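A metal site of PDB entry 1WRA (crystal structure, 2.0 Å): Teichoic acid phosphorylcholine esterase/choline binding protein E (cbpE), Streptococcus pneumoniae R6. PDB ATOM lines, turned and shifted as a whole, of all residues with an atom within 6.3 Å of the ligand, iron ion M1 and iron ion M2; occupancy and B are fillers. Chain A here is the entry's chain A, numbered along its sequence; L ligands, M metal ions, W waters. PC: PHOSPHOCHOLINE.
Water W5 binds iron ion M2 (2.1 Å).
The side-chain amide oxygen (OD1) of Asn 182 is bound to iron ion M2.
Iron ion M2 is bound by O4 of the ligand (2.2 Å).
Iron ion M2 is bound by a ring nitrogen (ND1) of His 86, 2.2 Å away.
Iron ion M2 is bound by OD2 of Asp 202 (2.3 Å).
A ring nitrogen (NE2) of His 84 is bound to iron ion M2, 2.4 Å away.
O of Gly 52 touches C5 of the ligand, 3.1 Å away.
Ser 87 touches the ligand.
Trp 122 touches the ligand (CE3 to C4, 3.6 Å).
Hydrophobic or aromatic side chains within 4 Å of the ligand: His 86, Trp 122, His 227 and His 228.
Nine residues have an atom within 4 Å of the ligand: Gly 52, His 86, Ser 87, Asp 88, Trp 122, Asn 182, Asp 202, His 227 and His 228.
Water W5 lies within hydrogen-bond range of the side-chain carboxylate of Asp 88 (2.6 Å) and an oxygen (O2) of the ligand (2.9 Å).
Water W4 lies within hydrogen-bond range of OD2 of Asp 180 (3.0 Å), NH1 of Arg 120 (3.1 Å) and ND2 of Asn 182 (3.4 Å).
Water W2 lies within hydrogen-bond range of the backbone NH of Ser 87 (2.9 Å) and the side-chain amide oxygen of Asn 124 (3.0 Å).
Water W1 lies within hydrogen-bond range of OG of Ser 87 (2.6 Å) and N of Glu 54 (2.9 Å).
A ring nitrogen (NE2) of His 227 is in hydrogen-bond range of an oxygen (O3) of the ligand.
Iron ion M1 is bound by NE2 of His 89 (2.1 Å), water W5 (2.2 Å), OD2 of Asp 88 (2.2 Å), OD2 of Asp 202 (2.2 Å), O1 of the ligand (2.2 Å) and NE2 of His 228 (2.2 Å).
The backbone NH (N) of Asn 182 lies within hydrogen-bond range of the side-chain carboxylate (OD1) of Asp 180 (2.9 Å).
The side-chain carboxylate of Glu 35 is in hydrogen-bond range of the backbone NH of Asp 88.
N of Asp 202 lies within hydrogen-bond range of OG of Ser 185, 3.0 Å away.
A ring nitrogen (ND1) of His 228 sits close to the backbone NH of Ser 17.
A ring nitrogen (ND1) of His 228 lies close to the side-chain carboxylate (OD1) of Asp 18 (3.5 Å).
The backbone carbonyl oxygen (O) of Asp 88 lies within hydrogen-bond range of the backbone NH (N) of Asp 18, at 3.1 Å.
A ring nitrogen (NE2) of His 227 sits close to the side-chain amide nitrogen of Asn 182 (3.4 Å).
OG of Ser 185 is in hydrogen-bond range of O of Asn 182, 2.8 Å away.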
ATOM      1  N   GLY A  16      21.731 -13.613 -17.192  1.00  0.00           N
ATOM      2  CA  GLY A  16      21.296 -12.932 -15.993  1.00  0.00           C
ATOM      3  C   GLY A  16      22.247 -11.798 -15.596  1.00  0.00           C
ATOM      4  O   GLY A  16      23.449 -11.948 -15.602  1.00  0.00           O
ATOM      5  N   SER A  17      21.671 -10.631 -15.305  1.00  0.00           N
ATOM      6  CA  SER A  17      22.439  -9.437 -14.955  1.00  0.00           C
ATOM      7  C   SER A  17      21.474  -8.407 -14.375  1.00  0.00           C
ATOM      8  O   SER A  17      20.321  -8.319 -14.782  1.00  0.00           O
ATOM      9  CB  SER A  17      23.182  -8.900 -16.221  1.00  0.00           C
ATOM     10  OG  SER A  17      23.824  -7.662 -15.956  1.00  0.00           O
ATOM     11  N   ASP A  18      21.924  -7.644 -13.393  1.00  0.00           N
ATOM     12  CA  ASP A  18      21.054  -6.686 -12.720  1.00  0.00           C
ATOM     13  C   ASP A  18      21.539  -5.268 -13.013  1.00  0.00           C
ATOM     14  O   ASP A  18      22.669  -4.928 -12.683  1.00  0.00           O
ATOM     15  CB  ASP A  18      21.178  -6.830 -11.206  1.00  0.00           C
ATOM     16  CG  ASP A  18      20.435  -8.003 -10.624  1.00  0.00           C
ATOM     17  OD1 ASP A  18      20.202  -9.020 -11.276  1.00  0.00           O
ATOM     18  OD2 ASP A  18      20.072  -7.954  -9.422  1.00  0.00           O
ATOM     19  N   GLU A  35      26.256  -5.853 -16.512  1.00  0.00           N
ATOM     20  CA  GLU A  35      27.475  -6.358 -17.092  1.00  0.00           C
ATOM     21  C   GLU A  35      27.994  -5.353 -18.141  1.00  0.00           C
ATOM     22  O   GLU A  35      27.187  -4.716 -18.846  1.00  0.00           O
ATOM     23  CB  GLU A  35      27.190  -7.698 -17.794  1.00  0.00           C
ATOM     24  CG  GLU A  35      28.405  -8.360 -18.442  1.00  0.00           C
ATOM     25  CD  GLU A  35      29.458  -8.716 -17.400  1.00  0.00           C
ATOM     26  OE1 GLU A  35      29.227  -9.707 -16.646  1.00  0.00           O
ATOM     27  OE2 GLU A  35      30.455  -7.944 -17.280  1.00  0.00           O
ATOM     28  N   GLY A  52      35.654 -18.684 -16.883  1.00  0.00           N
ATOM     29  CA  GLY A  52      34.327 -18.190 -16.541  1.00  0.00           C
ATOM     30  C   GLY A  52      34.167 -16.679 -16.375  1.00  0.00           C
ATOM     31  O   GLY A  52      33.050 -16.171 -16.183  1.00  0.00           O
ATOM     32  N   ILE A  53      35.267 -15.938 -16.411  1.00  0.00           N
ATOM     33  CA  ILE A  53      35.170 -14.483 -16.523  1.00  0.00           C
ATOM     34  C   ILE A  53      34.302 -14.178 -17.748  1.00  0.00           C
ATOM     35  O   ILE A  53      34.504 -14.703 -18.800  1.00  0.00           O
ATOM     36  CB  ILE A  53      36.556 -13.835 -16.683  1.00  0.00           C
ATOM     37  CG1 ILE A  53      37.302 -13.853 -15.323  1.00  0.00           C
ATOM     38  CG2 ILE A  53      36.420 -12.403 -17.275  1.00  0.00           C
ATOM     39  CD1 ILE A  53      38.706 -13.225 -15.347  1.00  0.00           C
ATOM     40  N   GLU A  54      33.345 -13.303 -17.587  1.00  0.00           N
ATOM     41  CA  GLU A  54      32.473 -12.998 -18.690  1.00  0.00           C
ATOM     42  C   GLU A  54      33.002 -12.081 -19.800  1.00  0.00           C
ATOM     43  O   GLU A  54      33.679 -11.097 -19.517  1.00  0.00           O
ATOM     44  CB  GLU A  54      31.242 -12.259 -18.150  1.00  0.00           C
ATOM     45  CG  GLU A  54      30.216 -11.822 -19.211  1.00  0.00           C
ATOM     46  CD  GLU A  54      29.526 -13.032 -19.774  1.00  0.00           C
ATOM     47  OE1 GLU A  54      29.905 -13.515 -20.870  1.00  0.00           O
ATOM     48  OE2 GLU A  54      28.659 -13.549 -19.064  1.00  0.00           O
ATOM     49  N   HIS A  84      27.153  -6.395  -4.847  1.00  0.00           N
ATOM     50  CA  HIS A  84      28.282  -7.306  -4.670  1.00  0.00           C
ATOM     51  C   HIS A  84      29.193  -7.117  -5.890  1.00  0.00           C
ATOM     52  O   HIS A  84      28.832  -6.329  -6.784  1.00  0.00           O
ATOM     53  CB  HIS A  84      27.857  -8.779  -4.420  1.00  0.00           C
ATOM     54  CG  HIS A  84      27.204  -9.450  -5.594  1.00  0.00           C
ATOM     55  ND1 HIS A  84      26.082  -8.954  -6.195  1.00  0.00           N
ATOM     56  CD2 HIS A  84      27.490 -10.624  -6.235  1.00  0.00           C
ATOM     57  CE1 HIS A  84      25.724  -9.754  -7.182  1.00  0.00           C
ATOM     58  NE2 HIS A  84      26.552 -10.789  -7.219  1.00  0.00           N
ATOM     59  N   HIS A  86      30.446  -9.096  -8.453  1.00  0.00           N
ATOM     60  CA  HIS A  86      30.321  -9.768  -9.721  1.00  0.00           C
ATOM     61  C   HIS A  86      30.025  -8.788 -10.859  1.00  0.00           C
ATOM     62  O   HIS A  86      29.222  -7.864 -10.725  1.00  0.00           O
ATOM     63  CB  HIS A  86      29.307 -10.935  -9.671  1.00  0.00           C
ATOM     64  CG  HIS A  86      29.672 -11.977  -8.675  1.00  0.00           C
ATOM     65  ND1 HIS A  86      28.752 -12.808  -8.074  1.00  0.00           N
ATOM     66  CD2 HIS A  86      30.887 -12.319  -8.159  1.00  0.00           C
ATOM     67  CE1 HIS A  86      29.379 -13.609  -7.225  1.00  0.00           C
ATOM     68  NE2 HIS A  86      30.675 -13.343  -7.274  1.00  0.00           N
ATOM     69  N   SER A  87      30.698  -9.052 -11.959  1.00  0.00           N
ATOM     70  CA  SER A  87      30.751  -8.171 -13.126  1.00  0.00           C
ATOM     71  C   SER A  87      29.370  -7.820 -13.692  1.00  0.00           C
ATOM     72  O   SER A  87      29.155  -6.694 -14.204  1.00  0.00           O
ATOM     73  CB  SER A  87      31.607  -8.838 -14.211  1.00  0.00           C
ATOM     74  OG  SER A  87      31.041 -10.091 -14.652  1.00  0.00           O
ATOM     75  N   ASP A  88      28.433  -8.764 -13.590  1.00  0.00           N
ATOM     76  CA  ASP A  88      27.057  -8.558 -14.075  1.00  0.00           C
ATOM     77  C   ASP A  88      26.196  -7.667 -13.145  1.00  0.00           C
ATOM     78  O   ASP A  88      24.989  -7.460 -13.375  1.00  0.00           O
ATOM     79  CB  ASP A  88      26.375  -9.916 -14.371  1.00  0.00           C
ATOM     80  CG  ASP A  88      26.266 -10.807 -13.140  1.00  0.00           C
ATOM     81  OD1 ASP A  88      27.324 -11.184 -12.554  1.00  0.00           O
ATOM     82  OD2 ASP A  88      25.147 -11.143 -12.692  1.00  0.00           O
ATOM     83  N   HIS A  89      26.850  -7.096 -12.131  1.00  0.00           N
ATOM     84  CA  HIS A  89      26.230  -6.130 -11.205  1.00  0.00           C
ATOM     85  C   HIS A  89      27.044  -4.832 -11.115  1.00  0.00           C
ATOM     86  O   HIS A  89      26.469  -3.742 -11.209  1.00  0.00           O
ATOM     87  CB  HIS A  89      26.016  -6.786  -9.805  1.00  0.00           C
ATOM     88  CG  HIS A  89      25.180  -8.036  -9.885  1.00  0.00           C
ATOM     89  ND1 HIS A  89      23.803  -8.032  -9.724  1.00  0.00           N
ATOM     90  CD2 HIS A  89      25.520  -9.302 -10.205  1.00  0.00           C
ATOM     91  CE1 HIS A  89      23.339  -9.241  -9.987  1.00  0.00           C
ATOM     92  NE2 HIS A  89      24.352 -10.039 -10.241  1.00  0.00           N
ATOM     93  N   ARG A 120      35.906 -18.967  -7.748  1.00  0.00           N
ATOM     94  CA  ARG A 120      34.860 -17.959  -7.708  1.00  0.00           C
ATOM     95  C   ARG A 120      35.394 -16.522  -7.492  1.00  0.00           C
ATOM     96  O   ARG A 120      34.700 -15.663  -6.933  1.00  0.00           O
ATOM     97  CB  ARG A 120      33.821 -18.367  -6.630  1.00  0.00           C
ATOM     98  CG  ARG A 120      33.257 -19.804  -6.799  1.00  0.00           C
ATOM     99  CD  ARG A 120      31.943 -20.109  -6.021  1.00  0.00           C
ATOM    100  NE  ARG A 120      31.146 -21.147  -6.709  1.00  0.00           N
ATOM    101  CZ  ARG A 120      30.093 -20.962  -7.473  1.00  0.00           C
ATOM    102  NH1 ARG A 120      29.574 -19.768  -7.684  1.00  0.00           N
ATOM    103  NH2 ARG A 120      29.520 -22.019  -8.008  1.00  0.00           N
ATOM    104  N   TRP A 122      36.954 -14.932 -10.277  1.00  0.00           N
ATOM    105  CA  TRP A 122      36.806 -14.394 -11.599  1.00  0.00           C
ATOM    106  C   TRP A 122      37.504 -13.005 -11.751  1.00  0.00           C
ATOM    107  O   TRP A 122      38.708 -12.831 -11.524  1.00  0.00           O
ATOM    108  CB  TRP A 122      35.295 -14.310 -11.920  1.00  0.00           C
ATOM    109  CG  TRP A 122      34.650 -15.668 -11.934  1.00  0.00           C
ATOM    110  CD1 TRP A 122      34.921 -16.697 -12.798  1.00  0.00           C
ATOM    111  CD2 TRP A 122      33.606 -16.128 -11.071  1.00  0.00           C
ATOM    112  NE1 TRP A 122      34.107 -17.767 -12.529  1.00  0.00           N
ATOM    113  CE2 TRP A 122      33.309 -17.458 -11.451  1.00  0.00           C
ATOM    114  CE3 TRP A 122      32.916 -15.566  -9.983  1.00  0.00           C
ATOM    115  CZ2 TRP A 122      32.334 -18.229 -10.801  1.00  0.00           C
ATOM    116  CZ3 TRP A 122      31.952 -16.328  -9.335  1.00  0.00           C
ATOM    117  CH2 TRP A 122      31.654 -17.645  -9.759  1.00  0.00           C
ATOM    118  N   ASP A 123      36.586 -12.076 -11.965  1.00  0.00           N
ATOM    119  CA  ASP A 123      36.611 -10.720 -12.356  1.00  0.00           C
ATOM    120  C   ASP A 123      36.368  -9.738 -11.189  1.00  0.00           C
ATOM    121  O   ASP A 123      36.313  -8.506 -11.350  1.00  0.00           O
ATOM    122  CB  ASP A 123      35.312 -10.593 -13.347  1.00  0.00           C
ATOM    123  CG  ASP A 123      35.692  -9.828 -14.403  1.00  0.00           C
ATOM    124  OD1 ASP A 123      36.951  -9.699 -14.204  1.00  0.00           O
ATOM    125  OD2 ASP A 123      35.066  -9.246 -15.284  1.00  0.00           O
ATOM    126  N   ASN A 124      36.121 -10.294 -10.020  1.00  0.00           N
ATOM    127  CA  ASN A 124      35.516  -9.529  -8.935  1.00  0.00           C
ATOM    128  C   ASN A 124      36.385  -8.308  -8.541  1.00  0.00           C
ATOM    129  O   ASN A 124      35.912  -7.200  -8.447  1.00  0.00           O
ATOM    130  CB  ASN A 124      35.365 -10.389  -7.675  1.00  0.00           C
ATOM    131  CG  ASN A 124      34.603 -11.697  -7.891  1.00  0.00           C
ATOM    132  OD1 ASN A 124      33.964 -11.913  -8.934  1.00  0.00           O
ATOM    133  ND2 ASN A 124      34.670 -12.579  -6.857  1.00  0.00           N
ATOM    134  N   ASP A 180      31.248 -17.353  -1.650  1.00  0.00           N
ATOM    135  CA  ASP A 180      30.986 -16.631  -2.883  1.00  0.00           C
ATOM    136  C   ASP A 180      30.471 -15.254  -2.531  1.00  0.00           C
ATOM    137  O   ASP A 180      29.754 -15.117  -1.555  1.00  0.00           O
ATOM    138  CB  ASP A 180      29.904 -17.378  -3.685  1.00  0.00           C
ATOM    139  CG  ASP A 180      29.671 -16.770  -5.057  1.00  0.00           C
ATOM    140  OD1 ASP A 180      28.759 -15.929  -5.211  1.00  0.00           O
ATOM    141  OD2 ASP A 180      30.375 -17.083  -6.040  1.00  0.00           O
ATOM    142  N   ASP A 181      30.814 -14.242  -3.312  1.00  0.00           N
ATOM    143  CA  ASP A 181      30.351 -12.886  -2.991  1.00  0.00           C
ATOM    144  C   ASP A 181      28.825 -12.683  -2.989  1.00  0.00           C
ATOM    145  O   ASP A 181      28.302 -11.693  -2.432  1.00  0.00           O
ATOM    146  CB  ASP A 181      31.043 -11.837  -3.861  1.00  0.00           C
ATOM    147  CG  ASP A 181      31.294 -10.528  -3.131  1.00  0.00           C
ATOM    148  OD1 ASP A 181      31.480 -10.581  -1.898  1.00  0.00           O
ATOM    149  OD2 ASP A 181      31.300  -9.415  -3.713  1.00  0.00           O
ATOM    150  N   ASN A 182      28.098 -13.614  -3.610  1.00  0.00           N
ATOM    151  CA  ASN A 182      26.627 -13.578  -3.572  1.00  0.00           C
ATOM    152  C   ASN A 182      26.074 -13.468  -2.158  1.00  0.00           C
ATOM    153  O   ASN A 182      25.091 -12.725  -1.914  1.00  0.00           O
ATOM    154  CB  ASN A 182      26.030 -14.813  -4.270  1.00  0.00           C
ATOM    155  CG  ASN A 182      26.069 -14.723  -5.808  1.00  0.00           C
ATOM    156  OD1 ASN A 182      26.557 -13.747  -6.378  1.00  0.00           O
ATOM    157  ND2 ASN A 182      25.550 -15.775  -6.485  1.00  0.00           N
ATOM    158  N   SER A 185      25.548 -10.027  -0.552  1.00  0.00           N
ATOM    159  CA  SER A 185      24.708  -9.079  -1.298  1.00  0.00           C
ATOM    160  C   SER A 185      24.024  -8.038  -0.396  1.00  0.00           C
ATOM    161  O   SER A 185      23.366  -8.380   0.602  1.00  0.00           O
ATOM    162  CB  SER A 185      23.630  -9.809  -2.102  1.00  0.00           C
ATOM    163  OG  SER A 185      24.178 -10.450  -3.231  1.00  0.00           O
ATOM    164  N   ASP A 202      22.187 -10.909  -5.488  1.00  0.00           N
ATOM    165  CA  ASP A 202      22.257 -12.369  -5.666  1.00  0.00           C
ATOM    166  C   ASP A 202      22.274 -13.083  -4.303  1.00  0.00           C
ATOM    167  O   ASP A 202      22.871 -14.164  -4.155  1.00  0.00           O
ATOM    168  CB  ASP A 202      23.493 -12.782  -6.466  1.00  0.00           C
ATOM    169  CG  ASP A 202      23.412 -12.459  -7.956  1.00  0.00           C
ATOM    170  OD1 ASP A 202      22.368 -11.957  -8.436  1.00  0.00           O
ATOM    171  OD2 ASP A 202      24.361 -12.730  -8.745  1.00  0.00           O
ATOM    172  N   HIS A 227      19.363 -13.753  -7.333  1.00  0.00           N
ATOM    173  CA  HIS A 227      20.279 -14.494  -8.171  1.00  0.00           C
ATOM    174  C   HIS A 227      19.614 -15.001  -9.471  1.00  0.00           C
ATOM    175  O   HIS A 227      19.820 -16.160  -9.862  1.00  0.00           O
ATOM    176  CB  HIS A 227      20.932 -15.628  -7.372  1.00  0.00           C
ATOM    177  CG  HIS A 227      22.156 -16.226  -8.020  1.00  0.00           C
ATOM    178  ND1 HIS A 227      22.690 -17.428  -7.630  1.00  0.00           N
ATOM    179  CD2 HIS A 227      22.921 -15.785  -9.048  1.00  0.00           C
ATOM    180  CE1 HIS A 227      23.760 -17.693  -8.375  1.00  0.00           C
ATOM    181  NE2 HIS A 227      23.906 -16.732  -9.253  1.00  0.00           N
ATOM    182  N   HIS A 228      18.842 -14.110 -10.095  1.00  0.00           N
ATOM    183  CA  HIS A 228      18.350 -14.224 -11.478  1.00  0.00           C
ATOM    184  C   HIS A 228      17.246 -15.304 -11.709  1.00  0.00           C
ATOM    185  O   HIS A 228      16.123 -14.984 -12.161  1.00  0.00           O
ATOM    186  CB  HIS A 228      19.539 -14.479 -12.400  1.00  0.00           C
ATOM    187  CG  HIS A 228      20.654 -13.473 -12.262  1.00  0.00           C
ATOM    188  ND1 HIS A 228      20.552 -12.183 -12.718  1.00  0.00           N
ATOM    189  CD2 HIS A 228      21.889 -13.590 -11.724  1.00  0.00           C
ATOM    190  CE1 HIS A 228      21.674 -11.538 -12.467  1.00  0.00           C
ATOM    191  NE2 HIS A 228      22.500 -12.364 -11.856  1.00  0.00           N
HETATM  192  P1   PC L   1      26.124 -15.143 -10.556  1.00  0.00           P
HETATM  193  O1   PC L   1      24.962 -14.207 -11.212  1.00  0.00           O
HETATM  194  O3   PC L   1      25.763 -16.584 -10.852  1.00  0.00           O
HETATM  195  O4   PC L   1      26.511 -14.932  -9.059  1.00  0.00           O
HETATM  196  O2   PC L   1      27.509 -14.759 -11.343  1.00  0.00           O
HETATM  197  C1   PC L   1      27.992 -15.501 -12.447  1.00  0.00           C
HETATM  198  C2   PC L   1      29.519 -15.539 -12.504  1.00  0.00           C
HETATM  199  N1   PC L   1      30.248 -14.352 -13.087  1.00  0.00           N
HETATM  200  C3   PC L   1      29.378 -13.491 -13.941  1.00  0.00           C
HETATM  201  C4   PC L   1      30.833 -13.475 -12.023  1.00  0.00           C
HETATM  202  C5   PC L   1      31.383 -14.901 -13.897  1.00  0.00           C
HETATM  203 FE    FE M   1      24.469 -12.083 -10.842  1.00  0.00          FE
HETATM  204 FE    FE M   2      26.570 -12.897  -8.303  1.00  0.00          FE
HETATM  205  O   HOH W   1      32.843 -11.990 -14.996  1.00  0.00           O
HETATM  206  O   HOH W   2      32.835 -10.998 -11.507  1.00  0.00           O
HETATM  207  O   HOH W   3      24.574 -14.102 -14.134  1.00  0.00           O
HETATM  208  O   HOH W   4      28.231 -17.035  -8.069  1.00  0.00           O
HETATM  209  O   HOH W   5      26.551 -12.271 -10.306  1.00  0.00           O
